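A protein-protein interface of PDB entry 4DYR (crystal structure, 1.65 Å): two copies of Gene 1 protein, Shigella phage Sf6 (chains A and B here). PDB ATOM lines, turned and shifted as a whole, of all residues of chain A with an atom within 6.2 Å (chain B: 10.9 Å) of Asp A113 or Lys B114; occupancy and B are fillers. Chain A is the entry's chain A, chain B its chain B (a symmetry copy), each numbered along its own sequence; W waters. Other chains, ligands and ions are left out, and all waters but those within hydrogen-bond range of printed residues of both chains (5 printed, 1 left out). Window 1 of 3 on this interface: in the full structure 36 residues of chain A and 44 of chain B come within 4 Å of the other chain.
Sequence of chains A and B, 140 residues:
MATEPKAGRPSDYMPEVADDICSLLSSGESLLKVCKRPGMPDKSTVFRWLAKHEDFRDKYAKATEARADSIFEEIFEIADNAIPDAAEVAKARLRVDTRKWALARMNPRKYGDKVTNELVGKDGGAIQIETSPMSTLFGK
Of the 17 printed residues of chain B, 9 touch a printed residue of chain A.
Printed residues of chain B that touch a printed residue of chain A: Lys B110, Tyr B111, Gly B112, Asp B113, Lys B114, Val B115, Thr B116, Asn B117 and Glu B118.
Hydrophobic or aromatic side chains of chain A that line the printed part of chain B: Pro A108 and Val A115.
Among the printed residues, 14 pairs touch across the chains.
Among the printed residues, Asp or Glu carboxylates within 4 Å of a Lys or Arg side-chain nitrogen of the other chain: Arg A105 with Asp B113 (2.9 Å).
Water W4 bridges the backbone carbonyl oxygen (O) of Lys B110 and the backbone carbonyl oxygen (O) of Arg A105.
Water W3 bridges the side-chain carboxylate of Asp B113 (2.9 Å) and the guanidinium group of Arg A105 (3.3 Å).
Water W1 lies within hydrogen-bond range of O of Pro A108 (2.9 Å) and OG1 of Thr B116 (3.0 Å).
Water W2 bridges O of Thr B116 (3.0 Å) and O of Val A115 (3.4 Å).
Water W5 bridges OG1 of Thr B116 (3.1 Å) and O of Arg A109 (3.1 Å).
Arg A105 touches Tyr B111, but with the chains exchanged Tyr A111 does not touch Arg B105 (17.0 Å).
Arg A105 touches Gly B112, but with the chains exchanged Gly A112 does not touch Arg B105 (16.2 Å).
Arg A105 touches Asp B113, but with the chains exchanged Asp A113 does not touch Arg B105 (13.7 Å).
Gly A112 touches Lys B114, but with the chains exchanged Lys A114 does not touch Gly B112 (12.1 Å).
Of the 14 pairs that touch across the chains among the printed residues, none has its exchanged pair printed and touching as well.
Printed residues of chain B within 4 Å of Ala A104: Lys B114.
Arg A105 touches four residues of chain B.
Pro A108 touches one residue of chain B.
Gly A112 touches just one residue of chain B: Lys B114.
Of chain B, only Lys B114, Val B115 and Thr B116 come within 4 Å of Asp A113.
Lys A114 touches just one residue of chain B: Thr B116 (3.8 Å).
Arg B105 touches none of the printed residues of chain A.
Of the printed residues of chain A, Tyr B111 touches Arg A105 (2.8 Å).
Of the printed residues of chain A, Gly B112 touches Arg A105.
Lys B114 touches four residues of chain A.
Of the printed residues of chain A, Val B115 touches Asp A113 (3.6 Å).
Of the printed residues of chain A, Asn B117 touches Val A115 (3.3 Å).
Of the printed residues of chain A, Glu B118 touches Val A115 (2.8 Å).
Among the printed residues, pairs that only touch across the chains: Ala A104 with Lys B114 (3.4 Å), Arg A105 with Lys B110 (3.5 Å), Pro A108 with Lys B114 (3.8 Å), Gly A112 with Lys B114 (3.5 Å), Asp A113 with Val B115 (3.6 Å), Lys A114 with Thr B116 (3.8 Å) and Val A115 with Asn B117 (3.3 Å).
The backbone carbonyl oxygen (O) of Arg B109 sits at hydrogen-bond distance from the side-chain amino group (NZ) of Lys B114, at 2.7 Å.
N of Lys B110 lies within hydrogen-bond range of OD1 of Asn B107, 3.2 Å away.
The side-chain amino group (NZ) of Lys A114 lies within hydrogen-bond range of the backbone carbonyl oxygen (O) of Arg A109, 2.7 Å away.
The backbone carbonyl oxygen (O) of Asp A113 sits at hydrogen-bond distance from the backbone NH (N) of Thr B116.
The guanidinium group of Arg A105 is in salt-bridge range of the side-chain carboxylate of Asp B113 (2.9 Å).
O of Lys B114 lies within hydrogen-bond range of N of Asp A113 (2.9 Å).
The guanidinium group of Arg A105 lies within hydrogen-bond range of the backbone carbonyl oxygen of Tyr B111, at 2.8 Å.
The backbone NH (N) of Val A115 sits at hydrogen-bond distance from the backbone carbonyl oxygen (O) of Thr B116 (3.0 Å).
The backbone NH (N) of Glu B118 is in hydrogen-bond range of the backbone carbonyl oxygen (O) of Val A115, at 2.8 Å.
NH2 of Arg A105 lies within hydrogen-bond range of O of Gly B112 (3.4 Å).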
ATOM      1  N   ALA A 104      29.866   8.556  -0.798  1.00  0.00           N
ATOM      2  CA  ALA A 104      29.218   8.320   0.489  1.00  0.00           C
ATOM      3  C   ALA A 104      30.250   8.337   1.603  1.00  0.00           C
ATOM      4  O   ALA A 104      29.960   8.749   2.726  1.00  0.00           O
ATOM      5  CB  ALA A 104      28.475   6.988   0.478  1.00  0.00           C
ATOM      6  N   ARG A 105      31.465   7.908   1.281  1.00  0.00           N
ATOM      7  CA  ARG A 105      32.530   7.911   2.274  1.00  0.00           C
ATOM      8  C   ARG A 105      33.197   9.270   2.428  1.00  0.00           C
ATOM      9  O   ARG A 105      33.637   9.633   3.517  1.00  0.00           O
ATOM     10  CB  ARG A 105      33.548   6.826   1.971  1.00  0.00           C
ATOM     11  CG  ARG A 105      32.994   5.475   2.369  1.00  0.00           C
ATOM     12  CD  ARG A 105      32.891   4.529   1.219  1.00  0.00           C
ATOM     13  NE  ARG A 105      32.312   3.277   1.684  1.00  0.00           N
ATOM     14  CZ  ARG A 105      31.115   2.818   1.344  1.00  0.00           C
ATOM     15  NH1 ARG A 105      30.343   3.493   0.496  1.00  0.00           N
ATOM     16  NH2 ARG A 105      30.706   1.655   1.841  1.00  0.00           N
ATOM     17  N   PRO A 108      29.552  11.551   4.254  1.00  0.00           N
ATOM     18  CA  PRO A 108      28.424  10.666   4.566  1.00  0.00           C
ATOM     19  C   PRO A 108      27.113  11.406   4.770  1.00  0.00           C
ATOM     20  O   PRO A 108      26.060  10.906   4.363  1.00  0.00           O
ATOM     21  CB  PRO A 108      28.866   9.978   5.865  1.00  0.00           C
ATOM     22  CG  PRO A 108      30.359  10.011   5.811  1.00  0.00           C
ATOM     23  CD  PRO A 108      30.724  11.292   5.110  1.00  0.00           C
ATOM     24  N   ARG A 109      27.162  12.591   5.368  1.00  0.00           N
ATOM     25  CA  ARG A 109      25.940  13.340   5.635  1.00  0.00           C
ATOM     26  C   ARG A 109      25.236  13.696   4.334  1.00  0.00           C
ATOM     27  O   ARG A 109      24.013  13.626   4.244  1.00  0.00           O
ATOM     28  CB  ARG A 109      26.268  14.605   6.434  1.00  0.00           C
ATOM     29  CG  ARG A 109      25.066  15.423   6.860  1.00  0.00           C
ATOM     30  CD  ARG A 109      25.477  16.492   7.866  1.00  0.00           C
ATOM     31  NE  ARG A 109      26.491  17.397   7.327  1.00  0.00           N
ATOM     32  CZ  ARG A 109      27.082  18.363   8.026  1.00  0.00           C
ATOM     33  NH1 ARG A 109      26.764  18.552   9.300  1.00  0.00           N
ATOM     34  NH2 ARG A 109      27.992  19.139   7.452  1.00  0.00           N
ATOM     35  N   TYR A 111      26.073  12.441   0.989  1.00  0.00           N
ATOM     36  CA  TYR A 111      26.032  11.465  -0.097  1.00  0.00           C
ATOM     37  C   TYR A 111      25.739  10.031   0.350  1.00  0.00           C
ATOM     38  O   TYR A 111      25.716   9.116  -0.470  1.00  0.00           O
ATOM     39  CB  TYR A 111      27.338  11.529  -0.933  1.00  0.00           C
ATOM     40  CG  TYR A 111      27.516  12.867  -1.606  1.00  0.00           C
ATOM     41  CD1 TYR A 111      26.555  13.358  -2.497  1.00  0.00           C
ATOM     42  CD2 TYR A 111      28.623  13.653  -1.341  1.00  0.00           C
ATOM     43  CE1 TYR A 111      26.707  14.596  -3.114  1.00  0.00           C
ATOM     44  CE2 TYR A 111      28.783  14.894  -1.957  1.00  0.00           C
ATOM     45  CZ  TYR A 111      27.818  15.358  -2.833  1.00  0.00           C
ATOM     46  OH  TYR A 111      27.974  16.590  -3.447  1.00  0.00           O
ATOM     47  N   GLY A 112      25.545   9.824   1.648  1.00  0.00           N
ATOM     48  CA  GLY A 112      25.163   8.511   2.129  1.00  0.00           C
ATOM     49  C   GLY A 112      23.756   8.161   1.656  1.00  0.00           C
ATOM     50  O   GLY A 112      23.033   9.022   1.133  1.00  0.00           O
ATOM     51  N   ASP A 113      23.366   6.902   1.836  1.00  0.00           N
ATOM     52  CA  ASP A 113      22.038   6.436   1.457  1.00  0.00           C
ATOM     53  C   ASP A 113      20.983   7.138   2.297  1.00  0.00           C
ATOM     54  O   ASP A 113      21.245   7.541   3.425  1.00  0.00           O
ATOM     55  CB  ASP A 113      21.917   4.926   1.703  1.00  0.00           C
ATOM     56  CG  ASP A 113      22.512   4.077   0.585  1.00  0.00           C
ATOM     57  OD1 ASP A 113      23.003   4.611  -0.436  1.00  0.00           O
ATOM     58  OD2 ASP A 113      22.470   2.836   0.734  1.00  0.00           O
ATOM     59  N   LYS A 114      19.782   7.265   1.747  1.00  0.00           N
ATOM     60  CA  LYS A 114      18.707   7.975   2.420  1.00  0.00           C
ATOM     61  C   LYS A 114      17.508   7.058   2.471  1.00  0.00           C
ATOM     62  O   LYS A 114      17.033   6.612   1.428  1.00  0.00           O
ATOM     63  CB  LYS A 114      18.326   9.246   1.645  1.00  0.00           C
ATOM     64  CG  LYS A 114      19.504  10.149   1.295  1.00  0.00           C
ATOM     65  CD  LYS A 114      20.195  10.653   2.539  1.00  0.00           C
ATOM     66  CE  LYS A 114      21.309  11.628   2.166  1.00  0.00           C
ATOM     67  NZ  LYS A 114      21.977  12.111   3.379  1.00  0.00           N
ATOM     68  N   VAL A 115      17.020   6.775   3.677  1.00  0.00           N
ATOM     69  CA  VAL A 115      15.867   5.906   3.840  1.00  0.00           C
ATOM     70  C   VAL A 115      14.899   6.547   4.828  1.00  0.00           C
ATOM     71  O   VAL A 115      15.316   7.135   5.832  1.00  0.00           O
ATOM     72  CB  VAL A 115      16.284   4.515   4.384  1.00  0.00           C
ATOM     73  CG1 VAL A 115      15.061   3.606   4.508  1.00  0.00           C
ATOM     74  CG2 VAL A 115      17.351   3.862   3.492  1.00  0.00           C
ATOM     75  N   PHE B  72      41.726   3.140  -1.483  1.00  0.00           N
ATOM     76  CA  PHE B  72      40.605   4.034  -1.758  1.00  0.00           C
ATOM     77  C   PHE B  72      40.915   4.897  -2.975  1.00  0.00           C
ATOM     78  O   PHE B  72      40.034   5.168  -3.803  1.00  0.00           O
ATOM     79  CB  PHE B  72      40.302   4.904  -0.527  1.00  0.00           C
ATOM     80  CG  PHE B  72      39.118   5.816  -0.698  1.00  0.00           C
ATOM     81  CD1 PHE B  72      37.830   5.310  -0.629  1.00  0.00           C
ATOM     82  CD2 PHE B  72      39.303   7.171  -0.881  1.00  0.00           C
ATOM     83  CE1 PHE B  72      36.730   6.152  -0.779  1.00  0.00           C
ATOM     84  CE2 PHE B  72      38.204   8.022  -1.025  1.00  0.00           C
ATOM     85  CZ  PHE B  72      36.930   7.506  -0.970  1.00  0.00           C
ATOM     86  N   LYS B 100      36.417  -2.588  -2.580  1.00  0.00           N
ATOM     87  CA  LYS B 100      35.356  -1.902  -1.848  1.00  0.00           C
ATOM     88  C   LYS B 100      34.952  -2.723  -0.633  1.00  0.00           C
ATOM     89  O   LYS B 100      34.781  -2.195   0.472  1.00  0.00           O
ATOM     90  CB  LYS B 100      34.134  -1.648  -2.749  1.00  0.00           C
ATOM     91  CG  LYS B 100      34.371  -0.509  -3.755  1.00  0.00           C
ATOM     92  CD  LYS B 100      33.124  -0.153  -4.553  1.00  0.00           C
ATOM     93  CE  LYS B 100      32.433  -1.372  -5.103  1.00  0.00           C
ATOM     94  NZ  LYS B 100      31.246  -0.994  -5.911  1.00  0.00           N
ATOM     95  N   LEU B 103      37.850  -2.706   1.960  1.00  0.00           N
ATOM     96  CA  LEU B 103      38.010  -1.428   2.639  1.00  0.00           C
ATOM     97  C   LEU B 103      37.107  -1.290   3.857  1.00  0.00           C
ATOM     98  O   LEU B 103      37.537  -0.774   4.893  1.00  0.00           O
ATOM     99  CB  LEU B 103      37.736  -0.268   1.667  1.00  0.00           C
ATOM    100  CG  LEU B 103      38.977   0.340   0.994  1.00  0.00           C
ATOM    101  CD1 LEU B 103      40.035  -0.706   0.693  1.00  0.00           C
ATOM    102  CD2 LEU B 103      38.567   1.115  -0.274  1.00  0.00           C
ATOM    103  N   ALA B 104      35.861  -1.743   3.739  1.00  0.00           N
ATOM    104  CA  ALA B 104      34.916  -1.578   4.836  1.00  0.00           C
ATOM    105  C   ALA B 104      35.389  -2.389   6.043  1.00  0.00           C
ATOM    106  O   ALA B 104      35.169  -1.996   7.177  1.00  0.00           O
ATOM    107  CB  ALA B 104      33.506  -1.980   4.416  1.00  0.00           C
ATOM    108  N   ARG B 105      36.043  -3.515   5.787  1.00  0.00           N
ATOM    109  CA  ARG B 105      36.573  -4.332   6.876  1.00  0.00           C
ATOM    110  C   ARG B 105      37.862  -3.779   7.457  1.00  0.00           C
ATOM    111  O   ARG B 105      38.116  -3.909   8.659  1.00  0.00           O
ATOM    112  CB  ARG B 105      36.805  -5.766   6.422  1.00  0.00           C
ATOM    113  CG  ARG B 105      35.534  -6.582   6.472  1.00  0.00           C
ATOM    114  CD  ARG B 105      34.953  -6.728   5.114  1.00  0.00           C
ATOM    115  NE  ARG B 105      33.645  -7.361   5.184  1.00  0.00           N
ATOM    116  CZ  ARG B 105      32.570  -6.880   4.590  1.00  0.00           C
ATOM    117  NH1 ARG B 105      32.650  -5.779   3.852  1.00  0.00           N
ATOM    118  NH2 ARG B 105      31.412  -7.532   4.709  1.00  0.00           N
ATOM    119  N   ASN B 107      38.829  -0.594   7.613  1.00  0.00           N
ATOM    120  CA  ASN B 107      38.523   0.570   8.429  1.00  0.00           C
ATOM    121  C   ASN B 107      37.029   0.844   8.379  1.00  0.00           C
ATOM    122  O   ASN B 107      36.562   1.619   7.542  1.00  0.00           O
ATOM    123  CB  ASN B 107      39.330   1.782   7.937  1.00  0.00           C
ATOM    124  CG  ASN B 107      39.243   2.966   8.881  1.00  0.00           C
ATOM    125  OD1 ASN B 107      38.284   3.100   9.654  1.00  0.00           O
ATOM    126  ND2 ASN B 107      40.229   3.854   8.802  1.00  0.00           N
ATOM    127  N   PRO B 108      36.265   0.161   9.247  1.00  0.00           N
ATOM    128  CA  PRO B 108      34.798   0.236   9.239  1.00  0.00           C
ATOM    129  C   PRO B 108      34.265   1.635   9.453  1.00  0.00           C
ATOM    130  O   PRO B 108      33.280   2.020   8.811  1.00  0.00           O
ATOM    131  CB  PRO B 108      34.392  -0.664  10.416  1.00  0.00           C
ATOM    132  CG  PRO B 108      35.496  -1.642  10.521  1.00  0.00           C
ATOM    133  CD  PRO B 108      36.758  -0.886  10.161  1.00  0.00           C
ATOM    134  N   ARG B 109      34.901   2.392  10.341  1.00  0.00           N
ATOM    135  CA  ARG B 109      34.449   3.743  10.643  1.00  0.00           C
ATOM    136  C   ARG B 109      34.527   4.630   9.407  1.00  0.00           C
ATOM    137  O   ARG B 109      33.624   5.427   9.131  1.00  0.00           O
ATOM    138  CB  ARG B 109      35.297   4.328  11.768  1.00  0.00           C
ATOM    139  CG  ARG B 109      34.928   5.726  12.201  1.00  0.00           C
ATOM    140  CD  ARG B 109      35.569   6.045  13.549  1.00  0.00           C
ATOM    141  NE  ARG B 109      37.026   6.131  13.477  1.00  0.00           N
ATOM    142  CZ  ARG B 109      37.848   5.729  14.444  1.00  0.00           C
ATOM    143  NH1 ARG B 109      37.362   5.199  15.560  1.00  0.00           N
ATOM    144  NH2 ARG B 109      39.163   5.851  14.292  1.00  0.00           N
ATOM    145  N   LYS B 110      35.606   4.482   8.649  1.00  0.00           N
ATOM    146  CA  LYS B 110      35.825   5.338   7.493  1.00  0.00           C
ATOM    147  C   LYS B 110      35.131   4.825   6.232  1.00  0.00           C
ATOM    148  O   LYS B 110      34.557   5.605   5.462  1.00  0.00           O
ATOM    149  CB  LYS B 110      37.308   5.450   7.235  1.00  0.00           C
ATOM    150  CG  LYS B 110      37.698   6.605   6.377  1.00  0.00           C
ATOM    151  CD  LYS B 110      39.184   6.837   6.533  1.00  0.00           C
ATOM    152  CE  LYS B 110      39.659   7.945   5.628  1.00  0.00           C
ATOM    153  NZ  LYS B 110      41.135   8.069   5.722  1.00  0.00           N
ATOM    154  N   TYR B 111      35.192   3.515   6.017  1.00  0.00           N
ATOM    155  CA  TYR B 111      34.798   2.960   4.728  1.00  0.00           C
ATOM    156  C   TYR B 111      33.556   2.057   4.755  1.00  0.00           C
ATOM    157  O   TYR B 111      33.182   1.498   3.731  1.00  0.00           O
ATOM    158  CB  TYR B 111      35.986   2.229   4.068  1.00  0.00           C
ATOM    159  CG  TYR B 111      37.167   3.140   3.811  1.00  0.00           C
ATOM    160  CD1 TYR B 111      37.044   4.242   2.969  1.00  0.00           C
ATOM    161  CD2 TYR B 111      38.393   2.899   4.410  1.00  0.00           C
ATOM    162  CE1 TYR B 111      38.115   5.093   2.740  1.00  0.00           C
ATOM    163  CE2 TYR B 111      39.470   3.740   4.176  1.00  0.00           C
ATOM    164  CZ  TYR B 111      39.315   4.831   3.339  1.00  0.00           C
ATOM    165  OH  TYR B 111      40.377   5.674   3.096  1.00  0.00           O
ATOM    166  N   GLY B 112      32.920   1.919   5.917  1.00  0.00           N
ATOM    167  CA  GLY B 112      31.659   1.197   6.000  1.00  0.00           C
ATOM    168  C   GLY B 112      30.551   1.938   5.269  1.00  0.00           C
ATOM    169  O   GLY B 112      30.710   3.104   4.892  1.00  0.00           O
ATOM    170  N   ASP B 113      29.423   1.260   5.062  1.00  0.00           N
ATOM    171  CA  ASP B 113      28.284   1.880   4.423  1.00  0.00           C
ATOM    172  C   ASP B 113      27.770   3.034   5.284  1.00  0.00           C
ATOM    173  O   ASP B 113      27.924   3.027   6.512  1.00  0.00           O
ATOM    174  CB  ASP B 113      27.150   0.855   4.256  1.00  0.00           C
ATOM    175  CG  ASP B 113      27.372  -0.105   3.091  1.00  0.00           C
ATOM    176  OD1 ASP B 113      28.333   0.069   2.303  1.00  0.00           O
ATOM    177  OD2 ASP B 113      26.547  -1.035   2.963  1.00  0.00           O
ATOM    178  N   LYS B 114      27.132   4.003   4.635  1.00  0.00           N
ATOM    179  CA  LYS B 114      26.620   5.185   5.317  1.00  0.00           C
ATOM    180  C   LYS B 114      25.148   5.334   4.987  1.00  0.00           C
ATOM    181  O   LYS B 114      24.788   5.429   3.820  1.00  0.00           O
ATOM    182  CB  LYS B 114      27.359   6.440   4.848  1.00  0.00           C
ATOM    183  CG  LYS B 114      28.889   6.316   4.847  1.00  0.00           C
ATOM    184  CD  LYS B 114      29.431   6.172   6.246  1.00  0.00           C
ATOM    185  CE  LYS B 114      30.961   6.132   6.227  1.00  0.00           C
ATOM    186  NZ  LYS B 114      31.474   5.745   7.552  1.00  0.00           N
ATOM    187  N   VAL B 115      24.296   5.316   6.012  1.00  0.00           N
ATOM    188  CA  VAL B 115      22.864   5.441   5.798  1.00  0.00           C
ATOM    189  C   VAL B 115      22.298   6.430   6.795  1.00  0.00           C
ATOM    190  O   VAL B 115      22.681   6.420   7.966  1.00  0.00           O
ATOM    191  CB  VAL B 115      22.142   4.082   6.014  1.00  0.00           C
ATOM    192  CG1 VAL B 115      20.653   4.235   5.756  1.00  0.00           C
ATOM    193  CG2 VAL B 115      22.736   2.984   5.128  1.00  0.00           C
ATOM    194  N   THR B 116      21.393   7.296   6.326  1.00  0.00           N
ATOM    195  CA  THR B 116      20.584   8.105   7.232  1.00  0.00           C
ATOM    196  C   THR B 116      19.161   7.580   7.205  1.00  0.00           C
ATOM    197  O   THR B 116      18.552   7.524   6.143  1.00  0.00           O
ATOM    198  CB  THR B 116      20.582   9.572   6.814  1.00  0.00           C
ATOM    199  OG1 THR B 116      21.938  10.060   6.820  1.00  0.00           O
ATOM    200  CG2 THR B 116      19.701  10.407   7.763  1.00  0.00           C
ATOM    201  N   ASN B 117      18.660   7.153   8.362  1.00  0.00           N
ATOM    202  CA  ASN B 117      17.309   6.600   8.455  1.00  0.00           C
ATOM    203  C   ASN B 117      16.434   7.619   9.149  1.00  0.00           C
ATOM    204  O   ASN B 117      16.637   7.909  10.332  1.00  0.00           O
ATOM    205  CB  ASN B 117      17.303   5.317   9.299  1.00  0.00           C
ATOM    206  CG  ASN B 117      18.116   4.188   8.676  1.00  0.00           C
ATOM    207  OD1 ASN B 117      17.593   3.354   7.916  1.00  0.00           O
ATOM    208  ND2 ASN B 117      19.388   4.142   9.006  1.00  0.00           N
ATOM    209  N   GLU B 118      15.471   8.161   8.414  1.00  0.00           N
ATOM    210  CA  GLU B 118      14.468   9.027   8.995  1.00  0.00           C
ATOM    211  C   GLU B 118      13.396   8.093   9.535  1.00  0.00           C
ATOM    212  O   GLU B 118      12.732   7.406   8.762  1.00  0.00           O
ATOM    213  CB  GLU B 118      13.890   9.959   7.917  1.00  0.00           C
ATOM    214  CG  GLU B 118      12.711  10.796   8.410  1.00  0.00           C
ATOM    215  CD  GLU B 118      11.967  11.521   7.288  1.00  0.00           C
ATOM    216  OE1 GLU B 118      12.059  11.087   6.115  1.00  0.00           O
ATOM    217  OE2 GLU B 118      11.283  12.528   7.584  1.00  0.00           O
HETATM  218  O   HOH W   1      24.778   9.208   6.399  1.00  0.00           O
HETATM  219  O   HOH W   2      17.137   9.944   5.057  1.00  0.00           O
HETATM  220  O   HOH W   3      30.641  -1.366   3.205  1.00  0.00           O
HETATM  221  O   HOH W   4      33.751   8.133   5.841  1.00  0.00           O
HETATM  222  O   HOH W   5      22.207  13.115   6.763  1.00  0.00           O
